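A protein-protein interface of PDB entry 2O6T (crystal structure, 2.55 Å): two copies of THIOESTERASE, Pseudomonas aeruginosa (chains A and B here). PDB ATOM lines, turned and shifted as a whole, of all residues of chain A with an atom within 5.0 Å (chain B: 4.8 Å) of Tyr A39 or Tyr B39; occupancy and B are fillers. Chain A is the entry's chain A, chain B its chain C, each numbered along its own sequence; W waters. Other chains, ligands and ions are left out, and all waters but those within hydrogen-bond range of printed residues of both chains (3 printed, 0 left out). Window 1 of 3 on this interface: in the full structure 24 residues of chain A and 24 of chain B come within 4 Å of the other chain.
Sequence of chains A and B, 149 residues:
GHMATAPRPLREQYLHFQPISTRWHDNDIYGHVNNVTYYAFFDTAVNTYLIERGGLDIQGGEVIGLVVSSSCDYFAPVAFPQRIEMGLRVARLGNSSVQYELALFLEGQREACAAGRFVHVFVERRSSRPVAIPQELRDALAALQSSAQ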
ATOM      1  N   ASN A  35      19.268 -10.250  19.265  1.00  0.00           N
ATOM      2  CA  ASN A  35      19.812 -11.539  19.685  1.00  0.00           C
ATOM      3  C   ASN A  35      20.327 -12.342  18.499  1.00  0.00           C
ATOM      4  O   ASN A  35      21.310 -13.060  18.623  1.00  0.00           O
ATOM      5  CB  ASN A  35      18.758 -12.355  20.446  1.00  0.00           C
ATOM      6  CG  ASN A  35      17.462 -12.560  19.633  1.00  0.00           C
ATOM      7  OD1 ASN A  35      16.648 -11.633  19.469  1.00  0.00           O
ATOM      8  ND2 ASN A  35      17.289 -13.756  19.101  1.00  0.00           N
ATOM      9  N   VAL A  36      19.660 -12.239  17.344  1.00  0.00           N
ATOM     10  CA  VAL A  36      20.074 -13.030  16.196  1.00  0.00           C
ATOM     11  C   VAL A  36      21.469 -12.681  15.769  1.00  0.00           C
ATOM     12  O   VAL A  36      22.252 -13.582  15.462  1.00  0.00           O
ATOM     13  CB  VAL A  36      19.126 -12.896  14.995  1.00  0.00           C
ATOM     14  CG1 VAL A  36      19.588 -13.809  13.823  1.00  0.00           C
ATOM     15  CG2 VAL A  36      17.668 -13.299  15.406  1.00  0.00           C
ATOM     16  N   THR A  37      21.807 -11.387  15.762  1.00  0.00           N
ATOM     17  CA  THR A  37      23.140 -10.936  15.377  1.00  0.00           C
ATOM     18  C   THR A  37      24.291 -11.623  16.158  1.00  0.00           C
ATOM     19  O   THR A  37      25.384 -11.851  15.619  1.00  0.00           O
ATOM     20  CB  THR A  37      23.204  -9.432  15.487  1.00  0.00           C
ATOM     21  OG1 THR A  37      22.242  -8.876  14.560  1.00  0.00           O
ATOM     22  CG2 THR A  37      24.586  -8.887  15.143  1.00  0.00           C
ATOM     23  N   TYR A  38      24.067 -11.969  17.415  1.00  0.00           N
ATOM     24  CA  TYR A  38      25.094 -12.681  18.137  1.00  0.00           C
ATOM     25  C   TYR A  38      25.587 -13.942  17.407  1.00  0.00           C
ATOM     26  O   TYR A  38      26.803 -14.241  17.375  1.00  0.00           O
ATOM     27  CB  TYR A  38      24.636 -13.031  19.542  1.00  0.00           C
ATOM     28  CG  TYR A  38      24.596 -11.831  20.463  1.00  0.00           C
ATOM     29  CD1 TYR A  38      23.518 -10.945  20.406  1.00  0.00           C
ATOM     30  CD2 TYR A  38      25.609 -11.599  21.395  1.00  0.00           C
ATOM     31  CE1 TYR A  38      23.424  -9.918  21.231  1.00  0.00           C
ATOM     32  CE2 TYR A  38      25.532 -10.518  22.236  1.00  0.00           C
ATOM     33  CZ  TYR A  38      24.423  -9.686  22.148  1.00  0.00           C
ATOM     34  OH  TYR A  38      24.260  -8.599  22.971  1.00  0.00           O
ATOM     35  N   TYR A  39      24.653 -14.650  16.799  1.00  0.00           N
ATOM     36  CA  TYR A  39      24.973 -15.873  16.121  1.00  0.00           C
ATOM     37  C   TYR A  39      25.774 -15.552  14.892  1.00  0.00           C
ATOM     38  O   TYR A  39      26.700 -16.298  14.550  1.00  0.00           O
ATOM     39  CB  TYR A  39      23.679 -16.608  15.746  1.00  0.00           C
ATOM     40  CG  TYR A  39      23.002 -17.282  16.919  1.00  0.00           C
ATOM     41  CD1 TYR A  39      21.809 -16.764  17.442  1.00  0.00           C
ATOM     42  CD2 TYR A  39      23.540 -18.470  17.493  1.00  0.00           C
ATOM     43  CE1 TYR A  39      21.125 -17.415  18.482  1.00  0.00           C
ATOM     44  CE2 TYR A  39      22.876 -19.149  18.557  1.00  0.00           C
ATOM     45  CZ  TYR A  39      21.665 -18.599  19.037  1.00  0.00           C
ATOM     46  OH  TYR A  39      21.008 -19.174  20.070  1.00  0.00           O
ATOM     47  N   ALA A  40      25.454 -14.429  14.218  1.00  0.00           N
ATOM     48  CA  ALA A  40      26.319 -13.967  13.120  1.00  0.00           C
ATOM     49  C   ALA A  40      27.748 -13.718  13.624  1.00  0.00           C
ATOM     50  O   ALA A  40      28.705 -14.026  12.923  1.00  0.00           O
ATOM     51  CB  ALA A  40      25.764 -12.752  12.468  1.00  0.00           C
ATOM     52  N   PHE A  41      27.887 -13.172  14.831  1.00  0.00           N
ATOM     53  CA  PHE A  41      29.217 -12.998  15.437  1.00  0.00           C
ATOM     54  C   PHE A  41      29.908 -14.356  15.665  1.00  0.00           C
ATOM     55  O   PHE A  41      31.132 -14.503  15.411  1.00  0.00           O
ATOM     56  CB  PHE A  41      29.140 -12.243  16.783  1.00  0.00           C
ATOM     57  CG  PHE A  41      28.625 -10.832  16.684  1.00  0.00           C
ATOM     58  CD1 PHE A  41      28.843 -10.067  15.549  1.00  0.00           C
ATOM     59  CD2 PHE A  41      27.955 -10.265  17.749  1.00  0.00           C
ATOM     60  CE1 PHE A  41      28.392  -8.773  15.473  1.00  0.00           C
ATOM     61  CE2 PHE A  41      27.491  -8.963  17.699  1.00  0.00           C
ATOM     62  CZ  PHE A  41      27.714  -8.210  16.554  1.00  0.00           C
ATOM     63  N   PHE A  42      29.138 -15.349  16.135  1.00  0.00           N
ATOM     64  CA  PHE A  42      29.718 -16.690  16.309  1.00  0.00           C
ATOM     65  C   PHE A  42      30.271 -17.224  14.987  1.00  0.00           C
ATOM     66  O   PHE A  42      31.409 -17.678  14.922  1.00  0.00           O
ATOM     67  CB  PHE A  42      28.724 -17.710  16.898  1.00  0.00           C
ATOM     68  CG  PHE A  42      28.229 -17.365  18.270  1.00  0.00           C
ATOM     69  CD1 PHE A  42      28.800 -16.335  18.995  1.00  0.00           C
ATOM     70  CD2 PHE A  42      27.215 -18.133  18.860  1.00  0.00           C
ATOM     71  CE1 PHE A  42      28.332 -16.005  20.293  1.00  0.00           C
ATOM     72  CE2 PHE A  42      26.765 -17.866  20.169  1.00  0.00           C
ATOM     73  CZ  PHE A  42      27.299 -16.783  20.870  1.00  0.00           C
ATOM     74  N   ASP A  43      29.472 -17.154  13.937  1.00  0.00           N
ATOM     75  CA  ASP A  43      29.846 -17.735  12.650  1.00  0.00           C
ATOM     76  C   ASP A  43      31.118 -17.104  12.117  1.00  0.00           C
ATOM     77  O   ASP A  43      31.973 -17.789  11.546  1.00  0.00           O
ATOM     78  CB  ASP A  43      28.747 -17.436  11.632  1.00  0.00           C
ATOM     79  CG  ASP A  43      28.240 -18.640  10.967  1.00  0.00           C
ATOM     80  OD1 ASP A  43      28.760 -19.735  11.289  1.00  0.00           O
ATOM     81  OD2 ASP A  43      27.306 -18.502  10.129  1.00  0.00           O
ATOM     82  N   SER A  70      23.177 -24.992  17.674  1.00  0.00           N
ATOM     83  CA  SER A  70      23.809 -23.830  18.257  1.00  0.00           C
ATOM     84  C   SER A  70      22.926 -23.411  19.384  1.00  0.00           C
ATOM     85  O   SER A  70      21.739 -23.773  19.414  1.00  0.00           O
ATOM     86  CB  SER A  70      23.902 -22.699  17.222  1.00  0.00           C
ATOM     87  OG  SER A  70      22.588 -22.380  16.742  1.00  0.00           O
ATOM     88  N   SER A  71      23.480 -22.630  20.301  1.00  0.00           N
ATOM     89  CA  SER A  71      22.626 -22.030  21.292  1.00  0.00           C
ATOM     90  C   SER A  71      23.362 -20.872  21.913  1.00  0.00           C
ATOM     91  O   SER A  71      24.565 -20.768  21.774  1.00  0.00           O
ATOM     92  CB  SER A  71      22.247 -23.068  22.348  1.00  0.00           C
ATOM     93  OG  SER A  71      23.434 -23.496  22.960  1.00  0.00           O
ATOM     94  N   CYS A  72      22.646 -20.034  22.656  1.00  0.00           N
ATOM     95  CA  CYS A  72      23.267 -18.839  23.234  1.00  0.00           C
ATOM     96  C   CYS A  72      22.478 -18.372  24.449  1.00  0.00           C
ATOM     97  O   CYS A  72      21.238 -18.450  24.463  1.00  0.00           O
ATOM     98  CB  CYS A  72      23.250 -17.736  22.153  1.00  0.00           C
ATOM     99  SG  CYS A  72      24.064 -16.221  22.626  1.00  0.00           S
ATOM    100  N   TYR A  74      21.983 -14.920  26.939  1.00  0.00           N
ATOM    101  CA  TYR A  74      22.268 -13.498  26.933  1.00  0.00           C
ATOM    102  C   TYR A  74      22.251 -12.907  28.320  1.00  0.00           C
ATOM    103  O   TYR A  74      21.214 -13.005  29.034  1.00  0.00           O
ATOM    104  CB  TYR A  74      21.272 -12.770  26.057  1.00  0.00           C
ATOM    105  CG  TYR A  74      21.179 -13.353  24.674  1.00  0.00           C
ATOM    106  CD1 TYR A  74      20.340 -14.451  24.400  1.00  0.00           C
ATOM    107  CD2 TYR A  74      21.938 -12.810  23.621  1.00  0.00           C
ATOM    108  CE1 TYR A  74      20.283 -14.977  23.129  1.00  0.00           C
ATOM    109  CE2 TYR A  74      21.877 -13.330  22.351  1.00  0.00           C
ATOM    110  CZ  TYR A  74      21.051 -14.407  22.113  1.00  0.00           C
ATOM    111  OH  TYR A  74      20.971 -14.878  20.819  1.00  0.00           O
ATOM    112  N   ASN B  35      22.402 -20.690   8.961  1.00  0.00           N
ATOM    113  CA  ASN B  35      21.881 -21.052  10.272  1.00  0.00           C
ATOM    114  C   ASN B  35      21.414 -19.864  11.074  1.00  0.00           C
ATOM    115  O   ASN B  35      20.432 -19.967  11.802  1.00  0.00           O
ATOM    116  CB  ASN B  35      22.951 -21.782  11.061  1.00  0.00           C
ATOM    117  CG  ASN B  35      24.243 -20.970  11.189  1.00  0.00           C
ATOM    118  OD1 ASN B  35      25.098 -20.988  10.308  1.00  0.00           O
ATOM    119  ND2 ASN B  35      24.375 -20.259  12.282  1.00  0.00           N
ATOM    120  N   VAL B  36      22.081 -18.718  10.906  1.00  0.00           N
ATOM    121  CA  VAL B  36      21.740 -17.493  11.670  1.00  0.00           C
ATOM    122  C   VAL B  36      20.294 -17.105  11.386  1.00  0.00           C
ATOM    123  O   VAL B  36      19.538 -16.757  12.289  1.00  0.00           O
ATOM    124  CB  VAL B  36      22.772 -16.299  11.444  1.00  0.00           C
ATOM    125  CG1 VAL B  36      22.359 -15.023  12.195  1.00  0.00           C
ATOM    126  CG2 VAL B  36      24.178 -16.722  11.920  1.00  0.00           C
ATOM    127  N   THR B  37      19.891 -17.251  10.143  1.00  0.00           N
ATOM    128  CA  THR B  37      18.590 -16.765   9.689  1.00  0.00           C
ATOM    129  C   THR B  37      17.424 -17.492  10.341  1.00  0.00           C
ATOM    130  O   THR B  37      16.326 -16.897  10.464  1.00  0.00           O
ATOM    131  CB  THR B  37      18.521 -16.874   8.158  1.00  0.00           C
ATOM    132  OG1 THR B  37      19.696 -16.241   7.628  1.00  0.00           O
ATOM    133  CG2 THR B  37      17.272 -16.202   7.570  1.00  0.00           C
ATOM    134  N   TYR B  38      17.634 -18.750  10.768  1.00  0.00           N
ATOM    135  CA  TYR B  38      16.559 -19.467  11.407  1.00  0.00           C
ATOM    136  C   TYR B  38      16.077 -18.728  12.645  1.00  0.00           C
ATOM    137  O   TYR B  38      14.872 -18.699  12.930  1.00  0.00           O
ATOM    138  CB  TYR B  38      16.989 -20.877  11.780  1.00  0.00           C
ATOM    139  CG  TYR B  38      17.064 -21.829  10.586  1.00  0.00           C
ATOM    140  CD1 TYR B  38      18.083 -21.702   9.616  1.00  0.00           C
ATOM    141  CD2 TYR B  38      16.121 -22.847  10.426  1.00  0.00           C
ATOM    142  CE1 TYR B  38      18.156 -22.553   8.561  1.00  0.00           C
ATOM    143  CE2 TYR B  38      16.197 -23.735   9.350  1.00  0.00           C
ATOM    144  CZ  TYR B  38      17.216 -23.581   8.432  1.00  0.00           C
ATOM    145  OH  TYR B  38      17.291 -24.432   7.361  1.00  0.00           O
ATOM    146  N   TYR B  39      17.002 -18.118  13.386  1.00  0.00           N
ATOM    147  CA  TYR B  39      16.609 -17.419  14.587  1.00  0.00           C
ATOM    148  C   TYR B  39      15.864 -16.139  14.247  1.00  0.00           C
ATOM    149  O   TYR B  39      14.984 -15.724  15.020  1.00  0.00           O
ATOM    150  CB  TYR B  39      17.817 -17.096  15.429  1.00  0.00           C
ATOM    151  CG  TYR B  39      18.509 -18.291  16.029  1.00  0.00           C
ATOM    152  CD1 TYR B  39      19.668 -18.797  15.460  1.00  0.00           C
ATOM    153  CD2 TYR B  39      18.010 -18.899  17.204  1.00  0.00           C
ATOM    154  CE1 TYR B  39      20.328 -19.856  16.060  1.00  0.00           C
ATOM    155  CE2 TYR B  39      18.658 -19.965  17.804  1.00  0.00           C
ATOM    156  CZ  TYR B  39      19.814 -20.437  17.240  1.00  0.00           C
ATOM    157  OH  TYR B  39      20.454 -21.496  17.803  1.00  0.00           O
ATOM    158  N   ALA B  40      16.187 -15.521  13.095  1.00  0.00           N
ATOM    159  CA  ALA B  40      15.364 -14.388  12.605  1.00  0.00           C
ATOM    160  C   ALA B  40      13.943 -14.835  12.351  1.00  0.00           C
ATOM    161  O   ALA B  40      13.004 -14.128  12.704  1.00  0.00           O
ATOM    162  CB  ALA B  40      15.938 -13.732  11.383  1.00  0.00           C
ATOM    163  N   PHE B  41      13.794 -16.015  11.757  1.00  0.00           N
ATOM    164  CA  PHE B  41      12.500 -16.701  11.628  1.00  0.00           C
ATOM    165  C   PHE B  41      11.780 -16.929  12.983  1.00  0.00           C
ATOM    166  O   PHE B  41      10.565 -16.638  13.099  1.00  0.00           O
ATOM    167  CB  PHE B  41      12.651 -18.055  10.906  1.00  0.00           C
ATOM    168  CG  PHE B  41      13.176 -17.950   9.514  1.00  0.00           C
ATOM    169  CD1 PHE B  41      12.945 -16.811   8.748  1.00  0.00           C
ATOM    170  CD2 PHE B  41      13.871 -19.006   8.951  1.00  0.00           C
ATOM    171  CE1 PHE B  41      13.413 -16.716   7.424  1.00  0.00           C
ATOM    172  CE2 PHE B  41      14.370 -18.933   7.627  1.00  0.00           C
ATOM    173  CZ  PHE B  41      14.127 -17.786   6.859  1.00  0.00           C
ATOM    174  N   PHE B  42      12.512 -17.451  13.974  1.00  0.00           N
ATOM    175  CA  PHE B  42      11.935 -17.610  15.304  1.00  0.00           C
ATOM    176  C   PHE B  42      11.403 -16.266  15.815  1.00  0.00           C
ATOM    177  O   PHE B  42      10.236 -16.150  16.245  1.00  0.00           O
ATOM    178  CB  PHE B  42      12.956 -18.148  16.311  1.00  0.00           C
ATOM    179  CG  PHE B  42      13.428 -19.557  16.020  1.00  0.00           C
ATOM    180  CD1 PHE B  42      12.896 -20.292  14.963  1.00  0.00           C
ATOM    181  CD2 PHE B  42      14.359 -20.181  16.877  1.00  0.00           C
ATOM    182  CE1 PHE B  42      13.284 -21.595  14.712  1.00  0.00           C
ATOM    183  CE2 PHE B  42      14.732 -21.516  16.664  1.00  0.00           C
ATOM    184  CZ  PHE B  42      14.193 -22.217  15.565  1.00  0.00           C
ATOM    185  N   ASP B  43      12.259 -15.259  15.741  1.00  0.00           N
ATOM    186  CA  ASP B  43      11.975 -13.989  16.328  1.00  0.00           C
ATOM    187  C   ASP B  43      10.791 -13.331  15.654  1.00  0.00           C
ATOM    188  O   ASP B  43       9.987 -12.651  16.284  1.00  0.00           O
ATOM    189  CB  ASP B  43      13.212 -13.133  16.207  1.00  0.00           C
ATOM    190  CG  ASP B  43      13.365 -12.171  17.353  1.00  0.00           C
ATOM    191  OD1 ASP B  43      12.605 -12.316  18.369  1.00  0.00           O
ATOM    192  OD2 ASP B  43      14.257 -11.282  17.247  1.00  0.00           O
ATOM    193  N   SER B  70      18.298 -18.933  23.652  1.00  0.00           N
ATOM    194  CA  SER B  70      17.743 -19.631  22.465  1.00  0.00           C
ATOM    195  C   SER B  70      18.644 -20.741  21.983  1.00  0.00           C
ATOM    196  O   SER B  70      19.839 -20.790  22.321  1.00  0.00           O
ATOM    197  CB  SER B  70      17.553 -18.657  21.285  1.00  0.00           C
ATOM    198  OG  SER B  70      18.825 -18.138  20.880  1.00  0.00           O
ATOM    199  N   SER B  71      18.074 -21.589  21.136  1.00  0.00           N
ATOM    200  CA  SER B  71      18.833 -22.635  20.454  1.00  0.00           C
ATOM    201  C   SER B  71      18.044 -23.263  19.338  1.00  0.00           C
ATOM    202  O   SER B  71      16.871 -22.993  19.171  1.00  0.00           O
ATOM    203  CB  SER B  71      19.269 -23.713  21.415  1.00  0.00           C
ATOM    204  OG  SER B  71      18.126 -24.210  22.001  1.00  0.00           O
ATOM    205  N   CYS B  72      18.704 -24.131  18.584  1.00  0.00           N
ATOM    206  CA  CYS B  72      18.155 -24.690  17.373  1.00  0.00           C
ATOM    207  C   CYS B  72      19.023 -25.874  17.007  1.00  0.00           C
ATOM    208  O   CYS B  72      20.278 -25.844  17.209  1.00  0.00           O
ATOM    209  CB  CYS B  72      18.252 -23.628  16.273  1.00  0.00           C
ATOM    210  SG  CYS B  72      17.387 -24.062  14.759  1.00  0.00           S
ATOM    211  N   TYR B  74      19.471 -28.396  13.469  1.00  0.00           N
ATOM    212  CA  TYR B  74      19.118 -28.393  12.069  1.00  0.00           C
ATOM    213  C   TYR B  74      19.172 -29.797  11.464  1.00  0.00           C
ATOM    214  O   TYR B  74      20.211 -30.437  11.485  1.00  0.00           O
ATOM    215  CB  TYR B  74      20.052 -27.461  11.294  1.00  0.00           C
ATOM    216  CG  TYR B  74      20.221 -26.101  11.925  1.00  0.00           C
ATOM    217  CD1 TYR B  74      21.155 -25.900  12.941  1.00  0.00           C
ATOM    218  CD2 TYR B  74      19.451 -25.001  11.491  1.00  0.00           C
ATOM    219  CE1 TYR B  74      21.311 -24.681  13.531  1.00  0.00           C
ATOM    220  CE2 TYR B  74      19.617 -23.751  12.069  1.00  0.00           C
ATOM    221  CZ  TYR B  74      20.562 -23.607  13.091  1.00  0.00           C
ATOM    222  OH  TYR B  74      20.752 -22.387  13.685  1.00  0.00           O
HETATM  223  O   HOH W   1      23.530 -20.850  14.465  1.00  0.00           O
HETATM  224  O   HOH W   2      20.428 -26.937  20.032  1.00  0.00           O
HETATM  225  O   HOH W   3      18.471 -15.886  19.542  1.00  0.00           O
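Printed residues of chain A that touch a printed residue of chain B: Asn A35, Val A36, Tyr A39, Ala A40, Asp A43, Ser A70, Ser A71, Cys A72 and Tyr A74.
Hydrophobic or aromatic side chains of chain A within 4 Å of the printed part of chain B: Val A36, Tyr A39 and Tyr A74.
Of the 13 printed residues of chain B, 9 touch a printed residue of chain A.
Hydrophobic or aromatic side chains of chain B that line the printed part of chain A: Val B36, Tyr B39 and Tyr B74.
Among the printed residues, no Asp or Glu carboxylate lies within 4 Å of a Lys or Arg side-chain nitrogen of the other chain.
OD1 of Asn A35 lies close to OD2 of Asp B43, at 3.3 Å.
OH of Tyr B39 is in hydrogen-bond range of OH of Tyr A39, at 3.3 Å.
The side-chain hydroxyl (OH) of Tyr A39 lies within hydrogen-bond range of the side-chain hydroxyl (OG) of Ser B70, 2.5 Å away.
OD1 of Asn B35 lies close to OD2 of Asp A43, 3.3 Å away.
The side-chain hydroxyl (OH) of Tyr B39 lies within hydrogen-bond range of the side-chain hydroxyl (OG) of Ser A70 (2.5 Å).
N of Ser A70 is in hydrogen-bond range of O of Cys B72.
N of Cys A72 is in hydrogen-bond range of O of Ser B70, 2.9 Å away.
Water W1 lies within hydrogen-bond range of the side-chain amide nitrogen of Asn B35 (2.4 Å), the side-chain hydroxyl of Ser A70 (2.9 Å) and the side-chain hydroxyl of Tyr B74 (3.3 Å).
Water W3 lies within hydrogen-bond range of ND2 of Asn A35 (2.5 Å), OG of Ser B70 (2.6 Å) and OH of Tyr A74 (3.0 Å).
Water W2 lies within hydrogen-bond range of the backbone carbonyl oxygen (O) of Cys B72 (3.0 Å) and the backbone carbonyl oxygen (O) of Ser A70 (3.5 Å).
The backbone carbonyl oxygen (O) of Asn A35 sits at hydrogen-bond distance from the side-chain hydroxyl (OH) of Tyr A74 (2.9 Å).
The backbone NH (N) of Cys A72 is in hydrogen-bond range of the side-chain hydroxyl (OH) of Tyr A39 (3.2 Å).
OH of Tyr B74 sits at hydrogen-bond distance from O of Asn B35, 3.1 Å away.
OH of Tyr B39 sits at hydrogen-bond distance from N of Cys B72, at 3.3 Å.
Of chain B, only Val B36, Tyr B39, Ser B70 and Ser B71 come within 4 Å of Tyr A39.
Of the printed residues of chain B, Ala A40 touches Val B36 (3.5 Å).
Of the printed residues of chain B, Asp A43 touches Asn B35 (3.3 Å).
Of the printed residues of chain A, Asn B35 touches Asp A43.
Tyr B39 touches just these residues of chain A: Val A36 (3.6 Å), Tyr A39 (3.2 Å) and Ser A70 (2.5 Å).
The nearest residue of chain A that does not touch Tyr B39 is Ser A71 (4.1 Å).
The nearest printed residue of chain B that does not touch Tyr A74 is Tyr B39 (6.2 Å).
Among the printed residues, merely in contact across the chains: Ser A70 with Ser B71 (3.2 Å), Ser A71 with Ser B71 (3.2 Å), Ser A71 with Ser B70 (3.2 Å), Val A36 with Val B36 (3.3 Å), Ala A40 with Val B36 (3.5 Å), Val A36 with Ala B40 (3.5 Å), Val A36 with Tyr B39 (3.6 Å), Ser A70 with Tyr B74 (3.6 Å), Tyr A39 with Val B36 (3.6 Å), Tyr A74 with Ser B70 (3.9 Å) and Tyr A39 with Ser B71 (3.9 Å).
Val A36 touches Ala B40, and with the chains exchanged Ala A40 touches Val B36.
Tyr A39 touches Ser B70, and with the chains exchanged Ser A70 touches Tyr B39.
Ser A70 touches Ser B71, and with the chains exchanged Ser A71 touches Ser B70.
Ser A70 touches Tyr B74, and with the chains exchanged Tyr A74 touches Ser B70.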
